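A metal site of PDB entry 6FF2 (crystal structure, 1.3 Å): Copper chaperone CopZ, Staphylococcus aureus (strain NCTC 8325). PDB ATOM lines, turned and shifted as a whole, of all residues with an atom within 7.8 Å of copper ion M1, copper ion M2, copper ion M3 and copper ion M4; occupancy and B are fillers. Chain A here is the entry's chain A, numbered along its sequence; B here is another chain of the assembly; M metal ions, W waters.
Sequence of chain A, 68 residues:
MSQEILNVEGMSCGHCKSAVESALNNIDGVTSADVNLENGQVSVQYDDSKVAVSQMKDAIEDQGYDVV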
ATOM      1  N   GLY A  10      -6.835   4.365  15.178  1.00  0.00           N
ATOM      2  CA  GLY A  10      -8.003   4.918  14.469  1.00  0.00           C
ATOM      3  C   GLY A  10      -7.702   5.361  13.048  1.00  0.00           C
ATOM      4  O   GLY A  10      -8.617   5.727  12.318  1.00  0.00           O
ATOM      5  N   MET A  11      -6.441   5.356  12.622  1.00  0.00           N
ATOM      6  CA  MET A  11      -6.118   5.841  11.266  1.00  0.00           C
ATOM      7  C   MET A  11      -6.356   4.673  10.322  1.00  0.00           C
ATOM      8  O   MET A  11      -5.668   3.670  10.372  1.00  0.00           O
ATOM      9  CB  MET A  11      -4.668   6.343  11.154  1.00  0.00           C
ATOM     10  CG  MET A  11      -4.372   7.448  12.137  1.00  0.00           C
ATOM     11  SD  MET A  11      -2.678   8.043  11.923  1.00  0.00           S
ATOM     12  CE  MET A  11      -1.750   6.558  12.270  1.00  0.00           C
ATOM     13  N   SER A  12      -7.357   4.802   9.437  1.00  0.00           N
ATOM     14  CA  SER A  12      -7.751   3.626   8.640  1.00  0.00           C
ATOM     15  C   SER A  12      -7.463   3.692   7.192  1.00  0.00           C
ATOM     16  O   SER A  12      -7.673   2.700   6.526  1.00  0.00           O
ATOM     17  CB  SER A  12      -9.263   3.364   8.801  1.00  0.00           C
ATOM     18  OG  SER A  12      -9.972   4.501   8.417  1.00  0.00           O
ATOM     19  N   CYS A  13      -7.100   4.841   6.664  1.00  0.00           N
ATOM     20  CA  CYS A  13      -6.971   5.042   5.220  1.00  0.00           C
ATOM     21  C   CYS A  13      -6.127   6.250   4.902  1.00  0.00           C
ATOM     22  O   CYS A  13      -5.698   6.978   5.783  1.00  0.00           O
ATOM     23  CB  CYS A  13      -8.368   5.247   4.548  1.00  0.00           C
ATOM     24  SG  CYS A  13      -9.133   6.864   4.875  1.00  0.00           S
ATOM     25  N   GLY A  14      -5.857   6.453   3.609  1.00  0.00           N
ATOM     26  CA  GLY A  14      -5.117   7.613   3.132  1.00  0.00           C
ATOM     27  C   GLY A  14      -5.652   8.978   3.524  1.00  0.00           C
ATOM     28  O   GLY A  14      -4.881   9.902   3.706  1.00  0.00           O
ATOM     29  N   HIS A  15      -6.975   9.118   3.713  1.00  0.00           N
ATOM     30  CA  HIS A  15      -7.546  10.372   4.209  1.00  0.00           C
ATOM     31  C   HIS A  15      -7.113  10.667   5.661  1.00  0.00           C
ATOM     32  O   HIS A  15      -6.840  11.833   6.001  1.00  0.00           O
ATOM     33  CB  HIS A  15      -9.071  10.320   4.206  1.00  0.00           C
ATOM     34  CG  HIS A  15      -9.685  10.296   2.847  1.00  0.00           C
ATOM     35  ND1 HIS A  15     -10.496   9.258   2.445  1.00  0.00           N
ATOM     36  CD2 HIS A  15      -9.665  11.195   1.841  1.00  0.00           C
ATOM     37  CE1 HIS A  15     -10.911   9.508   1.206  1.00  0.00           C
ATOM     38  NE2 HIS A  15     -10.448  10.683   0.832  1.00  0.00           N
ATOM     39  N   CYS A  16      -7.052   9.606   6.476  1.00  0.00           N
ATOM     40  CA  CYS A  16      -6.630   9.718   7.884  1.00  0.00           C
ATOM     41  C   CYS A  16      -5.156  10.151   7.917  1.00  0.00           C
ATOM     42  O   CYS A  16      -4.776  11.100   8.631  1.00  0.00           O
ATOM     43  CB  CYS A  16      -6.768   8.405   8.646  1.00  0.00           C
ATOM     44  SG  CYS A  16      -8.485   7.874   8.859  1.00  0.00           S
ATOM     45  N   LYS A  17      -4.357   9.497   7.098  1.00  0.00           N
ATOM     46  CA  LYS A  17      -2.934   9.853   6.955  1.00  0.00           C
ATOM     47  C   LYS A  17      -2.777  11.312   6.604  1.00  0.00           C
ATOM     48  O   LYS A  17      -1.969  12.055   7.200  1.00  0.00           O
ATOM     49  CB  LYS A  17      -2.257   8.935   5.989  1.00  0.00           C
ATOM     50  CG  LYS A  17      -0.893   9.374   5.453  1.00  0.00           C
ATOM     51  CD  LYS A  17      -0.284   8.188   4.753  1.00  0.00           C
ATOM     52  CE  LYS A  17       0.984   8.528   4.003  1.00  0.00           C
ATOM     53  NZ  LYS A  17       2.140   8.684   4.909  1.00  0.00           N
ATOM     54  N   SER A  18      -3.497  11.781   5.605  1.00  0.00           N
ATOM     55  CA  SER A  18      -3.367  13.134   5.157  1.00  0.00           C
ATOM     56  C   SER A  18      -3.742  14.115   6.254  1.00  0.00           C
ATOM     57  O   SER A  18      -3.058  15.128   6.470  1.00  0.00           O
ATOM     58  CB  SER A  18      -4.220  13.320   3.921  1.00  0.00           C
ATOM     59  OG  SER A  18      -4.107  14.629   3.528  1.00  0.00           O
ATOM     60  N   ALA A  19      -4.819  13.816   6.960  1.00  0.00           N
ATOM     61  CA  ALA A  19      -5.306  14.707   7.995  1.00  0.00           C
ATOM     62  C   ALA A  19      -4.305  14.821   9.165  1.00  0.00           C
ATOM     63  O   ALA A  19      -4.159  15.911   9.736  1.00  0.00           O
ATOM     64  CB  ALA A  19      -6.655  14.231   8.517  1.00  0.00           C
ATOM     65  N   LEU A  37       0.464   3.745   7.984  1.00  0.00           N
ATOM     66  CA  LEU A  37      -0.897   3.243   8.238  1.00  0.00           C
ATOM     67  C   LEU A  37      -0.905   1.790   8.656  1.00  0.00           C
ATOM     68  O   LEU A  37      -1.818   1.353   9.351  1.00  0.00           O
ATOM     69  CB  LEU A  37      -1.784   3.404   6.987  1.00  0.00           C
ATOM     70  CG  LEU A  37      -2.230   4.829   6.713  1.00  0.00           C
ATOM     71  CD1 LEU A  37      -2.925   4.842   5.358  1.00  0.00           C
ATOM     72  CD2 LEU A  37      -3.147   5.365   7.798  1.00  0.00           C
ATOM     73  N   GLN A  63      -8.064  15.790  15.703  1.00  0.00           N
ATOM     74  CA  GLN A  63      -8.531  15.190  14.439  1.00  0.00           C
ATOM     75  C   GLN A  63      -9.360  13.927  14.658  1.00  0.00           C
ATOM     76  O   GLN A  63      -9.838  13.343  13.664  1.00  0.00           O
ATOM     77  CB  GLN A  63      -7.352  14.843  13.513  1.00  0.00           C
ATOM     78  CG  GLN A  63      -6.570  16.048  13.050  1.00  0.00           C
ATOM     79  CD  GLN A  63      -7.398  16.962  12.171  1.00  0.00           C
ATOM     80  OE1 GLN A  63      -8.058  16.515  11.215  1.00  0.00           O
ATOM     81  NE2 GLN A  63      -7.436  18.212  12.501  1.00  0.00           N
ATOM     82  N   TYR A  65      -8.442  10.989  16.566  1.00  0.00           N
ATOM     83  CA  TYR A  65      -7.697   9.726  16.765  1.00  0.00           C
ATOM     84  C   TYR A  65      -7.246   9.611  18.225  1.00  0.00           C
ATOM     85  O   TYR A  65      -7.291  10.567  18.938  1.00  0.00           O
ATOM     86  CB  TYR A  65      -6.475   9.695  15.781  1.00  0.00           C
ATOM     87  CG  TYR A  65      -6.919   9.878  14.366  1.00  0.00           C
ATOM     88  CD1 TYR A  65      -7.558   8.860  13.696  1.00  0.00           C
ATOM     89  CD2 TYR A  65      -6.814  11.077  13.737  1.00  0.00           C
ATOM     90  CE1 TYR A  65      -8.076   9.071  12.422  1.00  0.00           C
ATOM     91  CE2 TYR A  65      -7.306  11.302  12.477  1.00  0.00           C
ATOM     92  CZ  TYR A  65      -7.931  10.304  11.836  1.00  0.00           C
ATOM     93  OH  TYR A  65      -8.433  10.603  10.607  1.00  0.00           O
ATOM     94  N   GLY B  10     -14.445  -0.797   1.093  1.00  0.00           N
ATOM     95  CA  GLY B  10     -13.257   0.030   1.291  1.00  0.00           C
ATOM     96  C   GLY B  10     -13.485   1.305   2.052  1.00  0.00           C
ATOM     97  O   GLY B  10     -12.537   2.039   2.290  1.00  0.00           O
ATOM     98  N   MET B  11     -14.719   1.591   2.471  1.00  0.00           N
ATOM     99  CA  MET B  11     -15.008   2.849   3.144  1.00  0.00           C
ATOM    100  C   MET B  11     -14.779   2.589   4.612  1.00  0.00           C
ATOM    101  O   MET B  11     -15.477   1.823   5.234  1.00  0.00           O
ATOM    102  CB  MET B  11     -16.445   3.308   2.943  1.00  0.00           C
ATOM    103  CG  MET B  11     -16.796   3.564   1.478  1.00  0.00           C
ATOM    104  SD  MET B  11     -18.501   4.112   1.257  1.00  0.00           S
ATOM    105  CE  MET B  11     -19.426   2.761   1.993  1.00  0.00           C
ATOM    106  N   SER B  12     -13.809   3.264   5.183  1.00  0.00           N
ATOM    107  CA  SER B  12     -13.350   2.817   6.499  1.00  0.00           C
ATOM    108  C   SER B  12     -13.570   3.851   7.585  1.00  0.00           C
ATOM    109  O   SER B  12     -13.327   3.567   8.763  1.00  0.00           O
ATOM    110  CB  SER B  12     -11.835   2.465   6.460  1.00  0.00           C
ATOM    111  OG  SER B  12     -11.079   3.564   6.120  1.00  0.00           O
ATOM    112  N   CYS B  13     -13.933   5.070   7.241  1.00  0.00           N
ATOM    113  CA  CYS B  13     -14.068   6.136   8.210  1.00  0.00           C
ATOM    114  C   CYS B  13     -14.936   7.269   7.700  1.00  0.00           C
ATOM    115  O   CYS B  13     -15.318   7.287   6.530  1.00  0.00           O
ATOM    116  CB  CYS B  13     -12.670   6.700   8.565  1.00  0.00           C
ATOM    117  SG  CYS B  13     -11.881   7.709   7.354  1.00  0.00           S
ATOM    118  N   GLY B  14     -15.095   8.265   8.522  1.00  0.00           N
ATOM    119  CA  GLY B  14     -15.874   9.420   8.184  1.00  0.00           C
ATOM    120  C   GLY B  14     -15.337  10.174   7.000  1.00  0.00           C
ATOM    121  O   GLY B  14     -16.089  10.846   6.290  1.00  0.00           O
ATOM    122  N   HIS B  15     -14.031  10.148   6.769  1.00  0.00           N
ATOM    123  CA  HIS B  15     -13.510  10.838   5.610  1.00  0.00           C
ATOM    124  C   HIS B  15     -13.938  10.137   4.333  1.00  0.00           C
ATOM    125  O   HIS B  15     -14.226  10.809   3.304  1.00  0.00           O
ATOM    126  CB  HIS B  15     -11.955  10.851   5.596  1.00  0.00           C
ATOM    127  CG  HIS B  15     -11.325  11.703   6.655  1.00  0.00           C
ATOM    128  ND1 HIS B  15     -10.521  11.162   7.637  1.00  0.00           N
ATOM    129  CD2 HIS B  15     -11.368  13.038   6.860  1.00  0.00           C
ATOM    130  CE1 HIS B  15     -10.072  12.145   8.402  1.00  0.00           C
ATOM    131  NE2 HIS B  15     -10.552  13.295   7.960  1.00  0.00           N
ATOM    132  N   CYS B  16     -13.934   8.809   4.368  1.00  0.00           N
ATOM    133  CA  CYS B  16     -14.409   8.031   3.202  1.00  0.00           C
ATOM    134  C   CYS B  16     -15.899   8.365   2.969  1.00  0.00           C
ATOM    135  O   CYS B  16     -16.305   8.521   1.797  1.00  0.00           O
ATOM    136  CB  CYS B  16     -14.254   6.551   3.400  1.00  0.00           C
ATOM    137  SG  CYS B  16     -12.559   5.964   3.628  1.00  0.00           S
ATOM    138  N   LYS B  17     -16.693   8.361   4.030  1.00  0.00           N
ATOM    139  CA  LYS B  17     -18.103   8.704   3.929  1.00  0.00           C
ATOM    140  C   LYS B  17     -18.289  10.038   3.286  1.00  0.00           C
ATOM    141  O   LYS B  17     -19.084  10.213   2.314  1.00  0.00           O
ATOM    142  CB  LYS B  17     -18.752   8.652   5.279  1.00  0.00           C
ATOM    143  CG  LYS B  17     -20.099   9.256   5.399  1.00  0.00           C
ATOM    144  CD  LYS B  17     -20.713   8.765   6.702  1.00  0.00           C
ATOM    145  CE  LYS B  17     -21.828   9.713   7.096  1.00  0.00           C
ATOM    146  NZ  LYS B  17     -23.106   9.188   6.621  1.00  0.00           N
ATOM    147  N   SER B  18     -17.563  11.057   3.749  1.00  0.00           N
ATOM    148  CA  SER B  18     -17.701  12.373   3.185  1.00  0.00           C
ATOM    149  C   SER B  18     -17.293  12.427   1.685  1.00  0.00           C
ATOM    150  O   SER B  18     -17.934  13.128   0.854  1.00  0.00           O
ATOM    151  CB  SER B  18     -16.856  13.312   4.058  1.00  0.00           C
ATOM    152  OG  SER B  18     -16.987  14.653   3.696  1.00  0.00           O
ATOM    153  N   ALA B  19     -16.199  11.740   1.310  1.00  0.00           N
ATOM    154  CA  ALA B  19     -15.695  11.693  -0.069  1.00  0.00           C
ATOM    155  C   ALA B  19     -16.733  11.125  -1.024  1.00  0.00           C
ATOM    156  O   ALA B  19     -16.946  11.674  -2.097  1.00  0.00           O
ATOM    157  CB  ALA B  19     -14.371  10.914  -0.181  1.00  0.00           C
ATOM    158  N   LEU B  37     -21.485   3.502   7.076  1.00  0.00           N
ATOM    159  CA  LEU B  37     -20.189   2.819   7.218  1.00  0.00           C
ATOM    160  C   LEU B  37     -20.243   1.445   7.870  1.00  0.00           C
ATOM    161  O   LEU B  37     -19.408   0.626   7.574  1.00  0.00           O
ATOM    162  CB  LEU B  37     -19.232   3.715   8.008  1.00  0.00           C
ATOM    163  CG  LEU B  37     -18.789   4.977   7.292  1.00  0.00           C
ATOM    164  CD1 LEU B  37     -18.099   5.873   8.301  1.00  0.00           C
ATOM    165  CD2 LEU B  37     -17.910   4.624   6.087  1.00  0.00           C
ATOM    166  N   GLN B  63     -13.268   7.435  -6.646  1.00  0.00           N
ATOM    167  CA  GLN B  63     -12.775   7.785  -5.338  1.00  0.00           C
ATOM    168  C   GLN B  63     -11.955   6.705  -4.676  1.00  0.00           C
ATOM    169  O   GLN B  63     -11.469   6.932  -3.546  1.00  0.00           O
ATOM    170  CB  GLN B  63     -13.931   8.206  -4.410  1.00  0.00           C
ATOM    171  CG  GLN B  63     -14.640   9.499  -4.799  1.00  0.00           C
ATOM    172  CD  GLN B  63     -13.753  10.690  -4.719  1.00  0.00           C
ATOM    173  OE1 GLN B  63     -13.130  10.941  -3.692  1.00  0.00           O
ATOM    174  NE2 GLN B  63     -13.636  11.400  -5.804  1.00  0.00           N
ATOM    175  N   TYR B  65     -12.978   3.275  -4.210  1.00  0.00           N
ATOM    176  CA  TYR B  65     -13.722   2.180  -3.540  1.00  0.00           C
ATOM    177  C   TYR B  65     -14.227   1.190  -4.586  1.00  0.00           C
ATOM    178  O   TYR B  65     -14.115   1.454  -5.746  1.00  0.00           O
ATOM    179  CB  TYR B  65     -14.869   2.754  -2.686  1.00  0.00           C
ATOM    180  CG  TYR B  65     -14.379   3.862  -1.796  1.00  0.00           C
ATOM    181  CD1 TYR B  65     -13.595   3.546  -0.678  1.00  0.00           C
ATOM    182  CD2 TYR B  65     -14.530   5.209  -2.110  1.00  0.00           C
ATOM    183  CE1 TYR B  65     -13.063   4.532   0.107  1.00  0.00           C
ATOM    184  CE2 TYR B  65     -13.984   6.194  -1.328  1.00  0.00           C
ATOM    185  CZ  TYR B  65     -13.244   5.813  -0.218  1.00  0.00           C
ATOM    186  OH  TYR B  65     -12.676   6.787   0.533  1.00  0.00           O
HETATM  187 CU    CU M   1     -10.661   7.415   3.225  1.00  0.00          CU
HETATM  188 CU    CU M   2      -9.479   7.156   7.013  1.00  0.00          CU
HETATM  189 CU    CU M   3     -10.416   9.246   8.265  1.00  0.00          CU
HETATM  190 CU    CU M   4     -11.585   6.603   5.488  1.00  0.00          CU
HETATM  191  O   HOH W   1      -9.660   5.851   1.276  1.00  0.00           O
HETATM  192  O   HOH W   2     -11.442   9.387  10.688  1.00  0.00           O
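Merely in contact with copper ion M1: Tyr 65 of chain B (3.4 Å).
Within 4 Å of copper ion M1: Cys 13 of chain A, His 15 of chain A, Cys 16 of chain B and Tyr 65 of chain B.
Merely in contact with copper ion M4: Ser 12 of chain A (3.9 Å) and Ser 12 of chain B (3.1 Å).
Five residues have an atom within 4 Å of copper ion M4: Ser 12 of chain A, Cys 13 of chain A, Ser 12 of chain B, Cys 13 of chain B and Cys 16 of chain B.
ND1 of His 15 of chain A binds copper ion M1, at 2.0 Å.
The side-chain sulfur (SG) of Cys 13 of chain A is bound to copper ion M1 (2.3 Å).
Copper ion M1 is bound by the side-chain sulfur (SG) of Cys 16 of chain B.
Copper ion M1 has three donor atoms within binding distance.
Slightly farther from copper ion M1 lies water W1 (2.7 Å).
The side-chain sulfur (SG) of Cys 16 of chain A lies close to the side-chain hydroxyl (OH) of Tyr 65 of chain A (3.2 Å).
OG of Ser 12 of chain B is in hydrogen-bond range of OG of Ser 12 of chain A (2.7 Å).
OH of Tyr 65 of chain B sits close to SG of Cys 16 of chain B (3.2 Å).
N of Ser 12 of chain A lies close to SG of Cys 16 of chain A, 3.3 Å away.
SG of Cys 16 of chain B sits close to N of Ser 12 of chain B.
Merely in contact with copper ion M2: Ser 12 of chain A (3.0 Å).
Of the 26 residues printed, 4 come within 4 Å of copper ion M2.
Along chain A the residues within 4 Å of copper ion M2 span positions 12 to 16.
Copper ion M2 is bound by SG of Cys 13 of chain A, at 2.2 Å.
The side-chain sulfur (SG) of Cys 16 of chain A binds copper ion M2, at 2.2 Å.
SG of Cys 13 of chain B binds copper ion M2, at 2.5 Å.
OH of Tyr 65 of chain A touches copper ion M3 (3.4 Å).
Within 4 Å of copper ion M3: Cys 16 of chain A, Tyr 65 of chain A, Cys 13 of chain B and His 15 of chain B.
The nearest printed residue that does not touch copper ion M3 is Cys 13 of chain A (4.3 Å).
Copper ion M4 is bound by the side-chain sulfur (SG) of Cys 13 of chain B (2.2 Å), the side-chain sulfur (SG) of Cys 16 of chain B (2.2 Å) and the side-chain sulfur (SG) of Cys 13 of chain A (2.5 Å).
A ring nitrogen (ND1) of His 15 of chain B is bound to copper ion M3, 2.0 Å away.
SG of Cys 13 of chain B binds copper ion M3.
Copper ion M3 is bound by SG of Cys 16 of chain A (2.4 Å).
Slightly farther from copper ion M3 lies water W2 (2.6 Å).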
